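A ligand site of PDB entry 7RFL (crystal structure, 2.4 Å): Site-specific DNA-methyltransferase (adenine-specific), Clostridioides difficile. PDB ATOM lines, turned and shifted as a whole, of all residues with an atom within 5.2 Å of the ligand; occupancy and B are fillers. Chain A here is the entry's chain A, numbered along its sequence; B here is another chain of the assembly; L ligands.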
ATOM      1  N   LYS A  26     -32.050  -1.446   4.871  1.00  0.00           N
ATOM      2  CA  LYS A  26     -32.761  -0.373   4.177  1.00  0.00           C
ATOM      3  C   LYS A  26     -34.277  -0.533   4.303  1.00  0.00           C
ATOM      4  O   LYS A  26     -35.004   0.463   4.232  1.00  0.00           O
ATOM      5  CB  LYS A  26     -32.348  -0.362   2.709  1.00  0.00           C
ATOM      6  CG  LYS A  26     -32.470  -1.718   2.032  1.00  0.00           C
ATOM      7  CD  LYS A  26     -31.222  -2.063   1.230  1.00  0.00           C
ATOM      8  CE  LYS A  26     -31.017  -1.099   0.071  1.00  0.00           C
ATOM      9  NZ  LYS A  26     -29.822  -1.451  -0.741  1.00  0.00           N
ATOM     10  N   ALA A  27     -34.753  -1.763   4.502  1.00  0.00           N
ATOM     11  CA  ALA A  27     -36.188  -1.987   4.678  1.00  0.00           C
ATOM     12  C   ALA A  27     -36.705  -1.421   5.989  1.00  0.00           C
ATOM     13  O   ALA A  27     -37.919  -1.226   6.129  1.00  0.00           O
ATOM     14  CB  ALA A  27     -36.497  -3.479   4.594  1.00  0.00           C
ATOM     15  N   TYR A  31     -32.776   4.998   6.623  1.00  0.00           N
ATOM     16  CA  TYR A  31     -32.183   5.776   5.542  1.00  0.00           C
ATOM     17  C   TYR A  31     -33.179   6.662   4.808  1.00  0.00           C
ATOM     18  O   TYR A  31     -32.769   7.458   3.963  1.00  0.00           O
ATOM     19  CB  TYR A  31     -31.494   4.836   4.538  1.00  0.00           C
ATOM     20  CG  TYR A  31     -30.431   3.952   5.148  1.00  0.00           C
ATOM     21  CD1 TYR A  31     -29.428   4.475   5.958  1.00  0.00           C
ATOM     22  CD2 TYR A  31     -30.426   2.577   4.907  1.00  0.00           C
ATOM     23  CE1 TYR A  31     -28.453   3.658   6.506  1.00  0.00           C
ATOM     24  CE2 TYR A  31     -29.452   1.760   5.456  1.00  0.00           C
ATOM     25  CZ  TYR A  31     -28.468   2.306   6.259  1.00  0.00           C
ATOM     26  OH  TYR A  31     -27.509   1.486   6.799  1.00  0.00           O
ATOM     27  N   TYR A  32     -34.474   6.526   5.097  1.00  0.00           N
ATOM     28  CA  TYR A  32     -35.485   7.401   4.527  1.00  0.00           C
ATOM     29  C   TYR A  32     -35.164   8.856   4.875  1.00  0.00           C
ATOM     30  O   TYR A  32     -35.009   9.203   6.051  1.00  0.00           O
ATOM     31  CB  TYR A  32     -36.862   7.005   5.056  1.00  0.00           C
ATOM     32  CG  TYR A  32     -38.011   7.949   4.724  1.00  0.00           C
ATOM     33  CD1 TYR A  32     -38.269   9.062   5.515  1.00  0.00           C
ATOM     34  CD2 TYR A  32     -38.846   7.706   3.638  1.00  0.00           C
ATOM     35  CE1 TYR A  32     -39.314   9.917   5.219  1.00  0.00           C
ATOM     36  CE2 TYR A  32     -39.892   8.557   3.333  1.00  0.00           C
ATOM     37  CZ  TYR A  32     -40.128   9.665   4.134  1.00  0.00           C
ATOM     38  OH  TYR A  32     -41.167  10.513   3.840  1.00  0.00           O
ATOM     39  N   ILE A  62     -29.999   9.548  -8.929  1.00  0.00           N
ATOM     40  CA  ILE A  62     -29.199   8.354  -9.192  1.00  0.00           C
ATOM     41  C   ILE A  62     -29.065   7.452  -7.975  1.00  0.00           C
ATOM     42  O   ILE A  62     -28.352   6.442  -8.030  1.00  0.00           O
ATOM     43  CB  ILE A  62     -27.781   8.714  -9.688  1.00  0.00           C
ATOM     44  CG1 ILE A  62     -27.079   9.627  -8.687  1.00  0.00           C
ATOM     45  CG2 ILE A  62     -27.845   9.383 -11.052  1.00  0.00           C
ATOM     46  CD1 ILE A  62     -25.653   9.934  -9.081  1.00  0.00           C
ATOM     47  N   SER A  63     -29.726   7.773  -6.870  1.00  0.00           N
ATOM     48  CA  SER A  63     -29.834   6.909  -5.697  1.00  0.00           C
ATOM     49  C   SER A  63     -31.278   6.900  -5.218  1.00  0.00           C
ATOM     50  O   SER A  63     -31.576   7.015  -4.032  1.00  0.00           O
ATOM     51  CB  SER A  63     -28.911   7.374  -4.575  1.00  0.00           C
ATOM     52  OG  SER A  63     -27.577   7.500  -5.035  1.00  0.00           O
ATOM     53  N   CYS A  64     -32.202   6.734  -6.168  1.00  0.00           N
ATOM     54  CA  CYS A  64     -33.598   7.080  -5.924  1.00  0.00           C
ATOM     55  C   CYS A  64     -34.230   6.197  -4.854  1.00  0.00           C
ATOM     56  O   CYS A  64     -35.175   6.622  -4.176  1.00  0.00           O
ATOM     57  CB  CYS A  64     -34.407   6.990  -7.222  1.00  0.00           C
ATOM     58  SG  CYS A  64     -34.458   5.340  -7.950  1.00  0.00           S
ATOM     59  N   GLY A  65     -33.722   4.972  -4.669  1.00  0.00           N
ATOM     60  CA  GLY A  65     -34.348   4.067  -3.723  1.00  0.00           C
ATOM     61  C   GLY A  65     -35.791   3.821  -4.119  1.00  0.00           C
ATOM     62  O   GLY A  65     -36.096   3.515  -5.278  1.00  0.00           O
ATOM     63  N   CYS A  66     -36.699   3.952  -3.161  1.00  0.00           N
ATOM     64  CA  CYS A  66     -38.121   3.799  -3.414  1.00  0.00           C
ATOM     65  C   CYS A  66     -38.772   5.086  -3.906  1.00  0.00           C
ATOM     66  O   CYS A  66     -39.989   5.109  -4.111  1.00  0.00           O
ATOM     67  CB  CYS A  66     -38.836   3.283  -2.168  1.00  0.00           C
ATOM     68  SG  CYS A  66     -38.476   1.550  -1.793  1.00  0.00           S
ATOM     69  N   ASN A  68     -38.284   8.597  -2.597  1.00  0.00           N
ATOM     70  CA  ASN A  68     -38.604   9.716  -1.709  1.00  0.00           C
ATOM     71  C   ASN A  68     -38.571  11.033  -2.469  1.00  0.00           C
ATOM     72  O   ASN A  68     -39.500  11.840  -2.391  1.00  0.00           O
ATOM     73  CB  ASN A  68     -37.622   9.748  -0.537  1.00  0.00           C
ATOM     74  CG  ASN A  68     -37.689   8.517   0.323  1.00  0.00           C
ATOM     75  OD1 ASN A  68     -38.419   7.573   0.037  1.00  0.00           O
ATOM     76  ND2 ASN A  68     -36.901   8.515   1.400  1.00  0.00           N
ATOM     77  N   ALA A 114     -32.295   6.110 -10.982  1.00  0.00           N
ATOM     78  CA  ALA A 114     -31.340   5.010 -11.069  1.00  0.00           C
ATOM     79  C   ALA A 114     -31.075   4.468  -9.677  1.00  0.00           C
ATOM     80  O   ALA A 114     -30.881   5.246  -8.725  1.00  0.00           O
ATOM     81  CB  ALA A 114     -30.023   5.464 -11.716  1.00  0.00           C
ATOM     82  N   ASP A 115     -31.077   3.143  -9.547  1.00  0.00           N
ATOM     83  CA  ASP A 115     -30.744   2.508  -8.280  1.00  0.00           C
ATOM     84  C   ASP A 115     -30.335   1.075  -8.550  1.00  0.00           C
ATOM     85  O   ASP A 115     -30.845   0.418  -9.472  1.00  0.00           O
ATOM     86  CB  ASP A 115     -31.922   2.553  -7.300  1.00  0.00           C
ATOM     87  CG  ASP A 115     -31.491   2.342  -5.860  1.00  0.00           C
ATOM     88  OD1 ASP A 115     -30.964   1.254  -5.554  1.00  0.00           O
ATOM     89  OD2 ASP A 115     -31.662   3.264  -5.049  1.00  0.00           O
ATOM     90  N   ILE A 116     -29.386   0.577  -7.747  1.00  0.00           N
ATOM     91  CA  ILE A 116     -28.842  -0.764  -7.962  1.00  0.00           C
ATOM     92  C   ILE A 116     -29.751  -1.854  -7.417  1.00  0.00           C
ATOM     93  O   ILE A 116     -29.591  -3.020  -7.796  1.00  0.00           O
ATOM     94  CB  ILE A 116     -27.432  -0.834  -7.331  1.00  0.00           C
ATOM     95  CG1 ILE A 116     -26.660  -2.054  -7.844  1.00  0.00           C
ATOM     96  CG2 ILE A 116     -27.519  -0.820  -5.807  1.00  0.00           C
ATOM     97  CD1 ILE A 116     -25.220  -2.090  -7.392  1.00  0.00           C
ATOM     98  N   ASP A 117     -30.731  -1.513  -6.581  1.00  0.00           N
ATOM     99  CA  ASP A 117     -31.620  -2.477  -5.954  1.00  0.00           C
ATOM    100  C   ASP A 117     -32.840  -2.684  -6.845  1.00  0.00           C
ATOM    101  O   ASP A 117     -33.627  -1.748  -7.067  1.00  0.00           O
ATOM    102  CB  ASP A 117     -32.034  -1.988  -4.568  1.00  0.00           C
ATOM    103  CG  ASP A 117     -32.767  -3.039  -3.747  1.00  0.00           C
ATOM    104  OD1 ASP A 117     -33.293  -4.005  -4.338  1.00  0.00           O
ATOM    105  OD2 ASP A 117     -32.816  -2.886  -2.510  1.00  0.00           O
ATOM    106  N   LYS A 119     -35.608  -4.421  -6.319  1.00  0.00           N
ATOM    107  CA  LYS A 119     -36.895  -4.295  -5.630  1.00  0.00           C
ATOM    108  C   LYS A 119     -37.263  -2.826  -5.439  1.00  0.00           C
ATOM    109  O   LYS A 119     -38.437  -2.460  -5.535  1.00  0.00           O
ATOM    110  CB  LYS A 119     -36.839  -5.035  -4.298  1.00  0.00           C
ATOM    111  CG  LYS A 119     -38.210  -5.270  -3.668  1.00  0.00           C
ATOM    112  CD  LYS A 119     -38.175  -6.406  -2.658  1.00  0.00           C
ATOM    113  CE  LYS A 119     -39.564  -6.733  -2.138  1.00  0.00           C
ATOM    114  NZ  LYS A 119     -39.570  -7.940  -1.279  1.00  0.00           N
ATOM    115  N   ALA A 120     -36.276  -1.979  -5.163  1.00  0.00           N
ATOM    116  CA  ALA A 120     -36.547  -0.550  -5.015  1.00  0.00           C
ATOM    117  C   ALA A 120     -37.055   0.045  -6.323  1.00  0.00           C
ATOM    118  O   ALA A 120     -38.017   0.827  -6.318  1.00  0.00           O
ATOM    119  CB  ALA A 120     -35.287   0.172  -4.546  1.00  0.00           C
ATOM    120  N   ILE A 123     -40.687  -1.120  -6.876  1.00  0.00           N
ATOM    121  CA  ILE A 123     -41.636  -0.412  -6.030  1.00  0.00           C
ATOM    122  C   ILE A 123     -41.839   1.022  -6.524  1.00  0.00           C
ATOM    123  O   ILE A 123     -42.961   1.539  -6.544  1.00  0.00           O
ATOM    124  CB  ILE A 123     -41.167  -0.445  -4.558  1.00  0.00           C
ATOM    125  CG1 ILE A 123     -41.237  -1.864  -4.012  1.00  0.00           C
ATOM    126  CG2 ILE A 123     -41.999   0.501  -3.700  1.00  0.00           C
ATOM    127  CD1 ILE A 123     -40.787  -1.994  -2.580  1.00  0.00           C
ATOM    128  N   CYS A 149     -29.201  -0.222 -12.087  1.00  0.00           N
ATOM    129  CA  CYS A 149     -27.805  -0.265 -12.521  1.00  0.00           C
ATOM    130  C   CYS A 149     -26.926   0.351 -11.441  1.00  0.00           C
ATOM    131  O   CYS A 149     -27.392   0.885 -10.438  1.00  0.00           O
ATOM    132  CB  CYS A 149     -27.608   0.476 -13.841  1.00  0.00           C
ATOM    133  SG  CYS A 149     -27.801   2.266 -13.700  1.00  0.00           S
ATOM    134  N   ASP A 150     -25.613   0.249 -11.676  1.00  0.00           N
ATOM    135  CA  ASP A 150     -24.610   0.988 -10.913  1.00  0.00           C
ATOM    136  C   ASP A 150     -24.472   2.359 -11.571  1.00  0.00           C
ATOM    137  O   ASP A 150     -23.929   2.467 -12.670  1.00  0.00           O
ATOM    138  CB  ASP A 150     -23.290   0.230 -10.902  1.00  0.00           C
ATOM    139  CG  ASP A 150     -22.238   0.867  -9.997  1.00  0.00           C
ATOM    140  OD1 ASP A 150     -22.249   2.105  -9.825  1.00  0.00           O
ATOM    141  OD2 ASP A 150     -21.391   0.123  -9.473  1.00  0.00           O
ATOM    142  N   SER A 151     -24.969   3.394 -10.892  1.00  0.00           N
ATOM    143  CA  SER A 151     -24.928   4.740 -11.465  1.00  0.00           C
ATOM    144  C   SER A 151     -23.499   5.202 -11.721  1.00  0.00           C
ATOM    145  O   SER A 151     -23.265   6.041 -12.600  1.00  0.00           O
ATOM    146  CB  SER A 151     -25.639   5.727 -10.547  1.00  0.00           C
ATOM    147  OG  SER A 151     -26.973   5.310 -10.274  1.00  0.00           O
ATOM    148  N   LEU A 152     -22.536   4.654 -10.985  1.00  0.00           N
ATOM    149  CA  LEU A 152     -21.139   5.013 -11.185  1.00  0.00           C
ATOM    150  C   LEU A 152     -20.492   4.270 -12.344  1.00  0.00           C
ATOM    151  O   LEU A 152     -19.409   4.662 -12.786  1.00  0.00           O
ATOM    152  CB  LEU A 152     -20.336   4.756  -9.899  1.00  0.00           C
ATOM    153  CG  LEU A 152     -20.793   5.569  -8.684  1.00  0.00           C
ATOM    154  CD1 LEU A 152     -19.844   5.354  -7.521  1.00  0.00           C
ATOM    155  CD2 LEU A 152     -20.911   7.044  -9.032  1.00  0.00           C
ATOM    156  N   ASN A 166     -30.135  11.569  -2.299  1.00  0.00           N
ATOM    157  CA  ASN A 166     -29.308  11.262  -1.140  1.00  0.00           C
ATOM    158  C   ASN A 166     -28.439  10.058  -1.487  1.00  0.00           C
ATOM    159  O   ASN A 166     -28.926   8.911  -1.460  1.00  0.00           O
ATOM    160  CB  ASN A 166     -30.183  10.980   0.078  1.00  0.00           C
ATOM    161  CG  ASN A 166     -29.380  10.612   1.316  1.00  0.00           C
ATOM    162  OD1 ASN A 166     -28.169  10.820   1.378  1.00  0.00           O
ATOM    163  ND2 ASN A 166     -30.071  10.076   2.321  1.00  0.00           N
ATOM    164  N   PRO A 167     -27.173  10.272  -1.831  1.00  0.00           N
ATOM    165  CA  PRO A 167     -26.321   9.173  -2.305  1.00  0.00           C
ATOM    166  C   PRO A 167     -25.947   8.244  -1.173  1.00  0.00           C
ATOM    167  O   PRO A 167     -26.124   8.582   0.009  1.00  0.00           O
ATOM    168  CB  PRO A 167     -25.095   9.903  -2.867  1.00  0.00           C
ATOM    169  CG  PRO A 167     -25.034  11.167  -2.069  1.00  0.00           C
ATOM    170  CD  PRO A 167     -26.464  11.557  -1.806  1.00  0.00           C
ATOM    171  N   PRO A 168     -25.439   7.047  -1.473  1.00  0.00           N
ATOM    172  CA  PRO A 168     -24.932   6.182  -0.406  1.00  0.00           C
ATOM    173  C   PRO A 168     -23.609   6.702   0.149  1.00  0.00           C
ATOM    174  O   PRO A 168     -22.781   7.254  -0.585  1.00  0.00           O
ATOM    175  CB  PRO A 168     -24.739   4.829  -1.104  1.00  0.00           C
ATOM    176  CG  PRO A 168     -24.527   5.182  -2.533  1.00  0.00           C
ATOM    177  CD  PRO A 168     -25.392   6.379  -2.789  1.00  0.00           C
ATOM    178  N   ILE A 170     -20.290   5.303   2.085  1.00  0.00           N
ATOM    179  CA  ILE A 170     -19.543   4.101   2.464  1.00  0.00           C
ATOM    180  C   ILE A 170     -18.075   4.476   2.614  1.00  0.00           C
ATOM    181  O   ILE A 170     -17.455   4.980   1.659  1.00  0.00           O
ATOM    182  CB  ILE A 170     -19.700   2.966   1.441  1.00  0.00           C
ATOM    183  CG1 ILE A 170     -21.167   2.555   1.297  1.00  0.00           C
ATOM    184  CG2 ILE A 170     -18.862   1.772   1.857  1.00  0.00           C
ATOM    185  CD1 ILE A 170     -21.415   1.494   0.243  1.00  0.00           C
ATOM    186  N   TYR A 179     -14.507  -3.353  -5.745  1.00  0.00           N
ATOM    187  CA  TYR A 179     -15.170  -2.090  -6.033  1.00  0.00           C
ATOM    188  C   TYR A 179     -14.263  -0.908  -5.723  1.00  0.00           C
ATOM    189  O   TYR A 179     -14.219   0.068  -6.479  1.00  0.00           O
ATOM    190  CB  TYR A 179     -16.479  -1.980  -5.253  1.00  0.00           C
ATOM    191  CG  TYR A 179     -17.459  -1.014  -5.872  1.00  0.00           C
ATOM    192  CD1 TYR A 179     -18.291  -1.414  -6.905  1.00  0.00           C
ATOM    193  CD2 TYR A 179     -17.552   0.301  -5.419  1.00  0.00           C
ATOM    194  CE1 TYR A 179     -19.188  -0.540  -7.483  1.00  0.00           C
ATOM    195  CE2 TYR A 179     -18.447   1.179  -5.988  1.00  0.00           C
ATOM    196  CZ  TYR A 179     -19.261   0.757  -7.014  1.00  0.00           C
ATOM    197  OH  TYR A 179     -20.158   1.631  -7.592  1.00  0.00           O
ATOM    198  N   LEU A 197     -17.357   6.928  -0.704  1.00  0.00           N
ATOM    199  CA  LEU A 197     -18.074   6.653  -1.941  1.00  0.00           C
ATOM    200  C   LEU A 197     -18.871   7.873  -2.421  1.00  0.00           C
ATOM    201  O   LEU A 197     -18.964   8.121  -3.635  1.00  0.00           O
ATOM    202  CB  LEU A 197     -18.993   5.453  -1.746  1.00  0.00           C
ATOM    203  CG  LEU A 197     -19.912   5.034  -2.901  1.00  0.00           C
ATOM    204  CD1 LEU A 197     -19.104   4.553  -4.090  1.00  0.00           C
ATOM    205  CD2 LEU A 197     -20.878   3.962  -2.445  1.00  0.00           C
ATOM    206  N   PHE A 201     -20.125   9.995  -6.104  1.00  0.00           N
ATOM    207  CA  PHE A 201     -21.458  10.399  -6.494  1.00  0.00           C
ATOM    208  C   PHE A 201     -21.533  11.903  -6.741  1.00  0.00           C
ATOM    209  O   PHE A 201     -22.221  12.350  -7.667  1.00  0.00           O
ATOM    210  CB  PHE A 201     -22.465   9.967  -5.428  1.00  0.00           C
ATOM    211  CG  PHE A 201     -22.999   8.581  -5.637  1.00  0.00           C
ATOM    212  CD1 PHE A 201     -22.295   7.475  -5.185  1.00  0.00           C
ATOM    213  CD2 PHE A 201     -24.196   8.375  -6.297  1.00  0.00           C
ATOM    214  CE1 PHE A 201     -22.776   6.190  -5.384  1.00  0.00           C
ATOM    215  CE2 PHE A 201     -24.690   7.105  -6.501  1.00  0.00           C
ATOM    216  CZ  PHE A 201     -23.976   6.009  -6.043  1.00  0.00           C
ATOM    217  P    DA B   8     -18.961   5.588   8.911  1.00  0.00           P
ATOM    218  OP1  DA B   8     -18.871   4.184   9.378  1.00  0.00           O
ATOM    219  OP2  DA B   8     -18.476   5.941   7.559  1.00  0.00           O
ATOM    220  O5'  DA B   8     -20.474   6.083   9.048  1.00  0.00           O
ATOM    221  C5'  DA B   8     -21.367   5.968   7.967  1.00  0.00           C
ATOM    222  C4'  DA B   8     -22.798   6.171   8.443  1.00  0.00           C
ATOM    223  O4'  DA B   8     -23.586   6.791   7.396  1.00  0.00           O
ATOM    224  C3'  DA B   8     -23.531   4.884   8.838  1.00  0.00           C
ATOM    225  O3'  DA B   8     -24.220   5.097  10.056  1.00  0.00           O
ATOM    226  C2'  DA B   8     -24.497   4.669   7.683  1.00  0.00           C
ATOM    227  C1'  DA B   8     -24.819   6.107   7.297  1.00  0.00           C
ATOM    228  N9   DA B   8     -25.320   6.275   5.946  1.00  0.00           N
ATOM    229  C8   DA B   8     -24.848   5.685   4.800  1.00  0.00           C
ATOM    230  N7   DA B   8     -25.498   6.019   3.720  1.00  0.00           N
ATOM    231  C5   DA B   8     -26.472   6.899   4.174  1.00  0.00           C
ATOM    232  C6   DA B   8     -27.488   7.617   3.512  1.00  0.00           C
ATOM    233  N6   DA B   8     -27.697   7.557   2.197  1.00  0.00           N
ATOM    234  N1   DA B   8     -28.289   8.408   4.271  1.00  0.00           N
ATOM    235  C2   DA B   8     -28.079   8.468   5.586  1.00  0.00           C
ATOM    236  N3   DA B   8     -27.157   7.844   6.320  1.00  0.00           N
ATOM    237  C4   DA B   8     -26.376   7.071   5.545  1.00  0.00           C
HETATM  238 BR1  LIG L   1     -23.371   1.448  -3.818  1.00  0.00          BR
HETATM  239  N1  LIG L   1     -23.575   2.194  -7.114  1.00  0.00           N
HETATM  240  C1  LIG L   1     -24.869   2.522  -6.979  1.00  0.00           C
HETATM  241  N2  LIG L   1     -25.535   2.928  -8.046  1.00  0.00           N
HETATM  242  C2  LIG L   1     -26.841   3.254  -7.886  1.00  0.00           C
HETATM  243  N3  LIG L   1     -27.552   3.222  -6.783  1.00  0.00           N
HETATM  244  C3  LIG L   1     -26.904   2.812  -5.678  1.00  0.00           C
HETATM  245  C4  LIG L   1     -25.525   2.451  -5.766  1.00  0.00           C
HETATM  246  C5  LIG L   1     -25.093   2.060  -4.464  1.00  0.00           C
HETATM  247  C6  LIG L   1     -26.201   2.198  -3.665  1.00  0.00           C
HETATM  248  N4  LIG L   1     -27.293   2.646  -4.375  1.00  0.00           N
HETATM  249  C7  LIG L   1     -28.608   2.906  -3.823  1.00  0.00           C
HETATM  250  O1  LIG L   1     -28.561   4.110  -3.084  1.00  0.00           O
HETATM  251  C8  LIG L   1     -29.359   3.966  -1.890  1.00  0.00           C
HETATM  252  C9  LIG L   1     -28.425   4.061  -0.649  1.00  0.00           C
HETATM  253  N5  LIG L   1     -28.904   4.981   0.407  1.00  0.00           N
HETATM  254  C10 LIG L   1     -29.898   5.951  -0.076  1.00  0.00           C
HETATM  255  C11 LIG L   1     -31.302   5.799   0.520  1.00  0.00           C
HETATM  256  C12 LIG L   1     -32.265   5.038  -0.374  1.00  0.00           C
HETATM  257  N6  LIG L   1     -33.645   5.195   0.036  1.00  0.00           N
HETATM  258  C13 LIG L   1     -34.473   4.132   0.127  1.00  0.00           C
HETATM  259  N7  LIG L   1     -33.864   2.936  -0.180  1.00  0.00           N
HETATM  260  C14 LIG L   1     -34.462   1.659  -0.183  1.00  0.00           C
HETATM  261  C15 LIG L   1     -35.426   1.346   0.762  1.00  0.00           C
HETATM  262  C16 LIG L   1     -36.009   0.099   0.776  1.00  0.00           C
HETATM  263  C17 LIG L   1     -35.632  -0.860  -0.143  1.00  0.00           C
HETATM  264  C18 LIG L   1     -36.297  -2.234  -0.099  1.00  0.00           C
HETATM  265  C19 LIG L   1     -35.295  -3.330   0.230  1.00  0.00           C
HETATM  266  C20 LIG L   1     -36.934  -2.509  -1.462  1.00  0.00           C
HETATM  267  C21 LIG L   1     -37.411  -2.235   0.946  1.00  0.00           C
HETATM  268  C22 LIG L   1     -34.657  -0.566  -1.092  1.00  0.00           C
HETATM  269  C23 LIG L   1     -34.070   0.698  -1.103  1.00  0.00           C
HETATM  270  O2  LIG L   1     -35.653   4.243   0.458  1.00  0.00           O
HETATM  271  C24 LIG L   1     -29.261   4.304   1.680  1.00  0.00           C
HETATM  272  C25 LIG L   1     -29.850   2.901   1.522  1.00  0.00           C
HETATM  273  C26 LIG L   1     -28.094   4.305   2.656  1.00  0.00           C
HETATM  274  C27 LIG L   1     -29.993   2.569  -1.919  1.00  0.00           C
HETATM  275  O3  LIG L   1     -31.330   2.606  -2.424  1.00  0.00           O
HETATM  276  C28 LIG L   1     -29.037   1.813  -2.844  1.00  0.00           C
HETATM  277  O4  LIG L   1     -29.723   0.751  -3.519  1.00  0.00           O
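The side-chain carboxylate of Asp 115 lies within hydrogen-bond range of the backbone NH of Asp 117 (3.0 Å). O of Asp 115 is in hydrogen-bond range of N of Cys 149 (3.2 Å). The backbone NH of Leu 152 sits at hydrogen-bond distance from the side-chain carboxylate of Asp 150 (2.8 Å). The side-chain carboxylate of Asp 117 is in salt-bridge range of the side-chain amino group of Lys 26, at 3.8 Å. N1 of DA 8 of chain B lies within hydrogen-bond range of the side-chain amide nitrogen of Asn 166, 3.1 Å away. The backbone carbonyl oxygen (O) of Cys 149 sits close to the backbone NH (N) of Ile 116, at 3.4 Å. The backbone carbonyl oxygen (O) of Ala 114 is in hydrogen-bond range of the backbone NH (N) of Ser 63, at 3.3 Å. The backbone NH (N) of Leu 197 lies within hydrogen-bond range of the backbone carbonyl oxygen (O) of Ile 170, at 3.1 Å.
Residues that only touch the ligand: Lys 26 (3.5 Å), Ala 27 (3.9 Å), Tyr 31 (3.4 Å), Ile 62 (3.5 Å), Ser 63 (3.6 Å), Gly 65 (3.6 Å), Cys 66 (3.8 Å), Asp 117 (3.3 Å), Lys 119 (3.8 Å), Ala 120 (3.6 Å), Cys 149 (3.5 Å), Asn 166 (3.4 Å), Pro 168 (3.6 Å), Leu 197 (3.8 Å) and Phe 201 (3.7 Å). Hydrophobic or aromatic side chains within 4 Å of the ligand: Ala 27, Tyr 31, Ile 116, Ala 120, Pro 168, Leu 197 and Phe 201. Of the 29 residues printed, 21 come within 4 Å of the ligand.
An oxygen (O4) of the ligand lies within hydrogen-bond range of the side-chain carboxylate of Asp 115, 2.4 Å away. The backbone NH of Ser 151 sits at hydrogen-bond distance from a nitrogen (N2) of the ligand (2.9 Å). A nitrogen (N1) of the ligand sits at hydrogen-bond distance from the side-chain carboxylate (OD1) of Asp 150 (3.0 Å). N6 of DA 8 of chain B lies close to a nitrogen (N5) of the ligand (3.4 Å). The backbone NH (N) of Ile 116 is in hydrogen-bond range of a nitrogen (N3) of the ligand (3.4 Å). The side-chain hydroxyl (OH) of Tyr 179 lies within hydrogen-bond range of a nitrogen (N1) of the ligand (3.5 Å).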
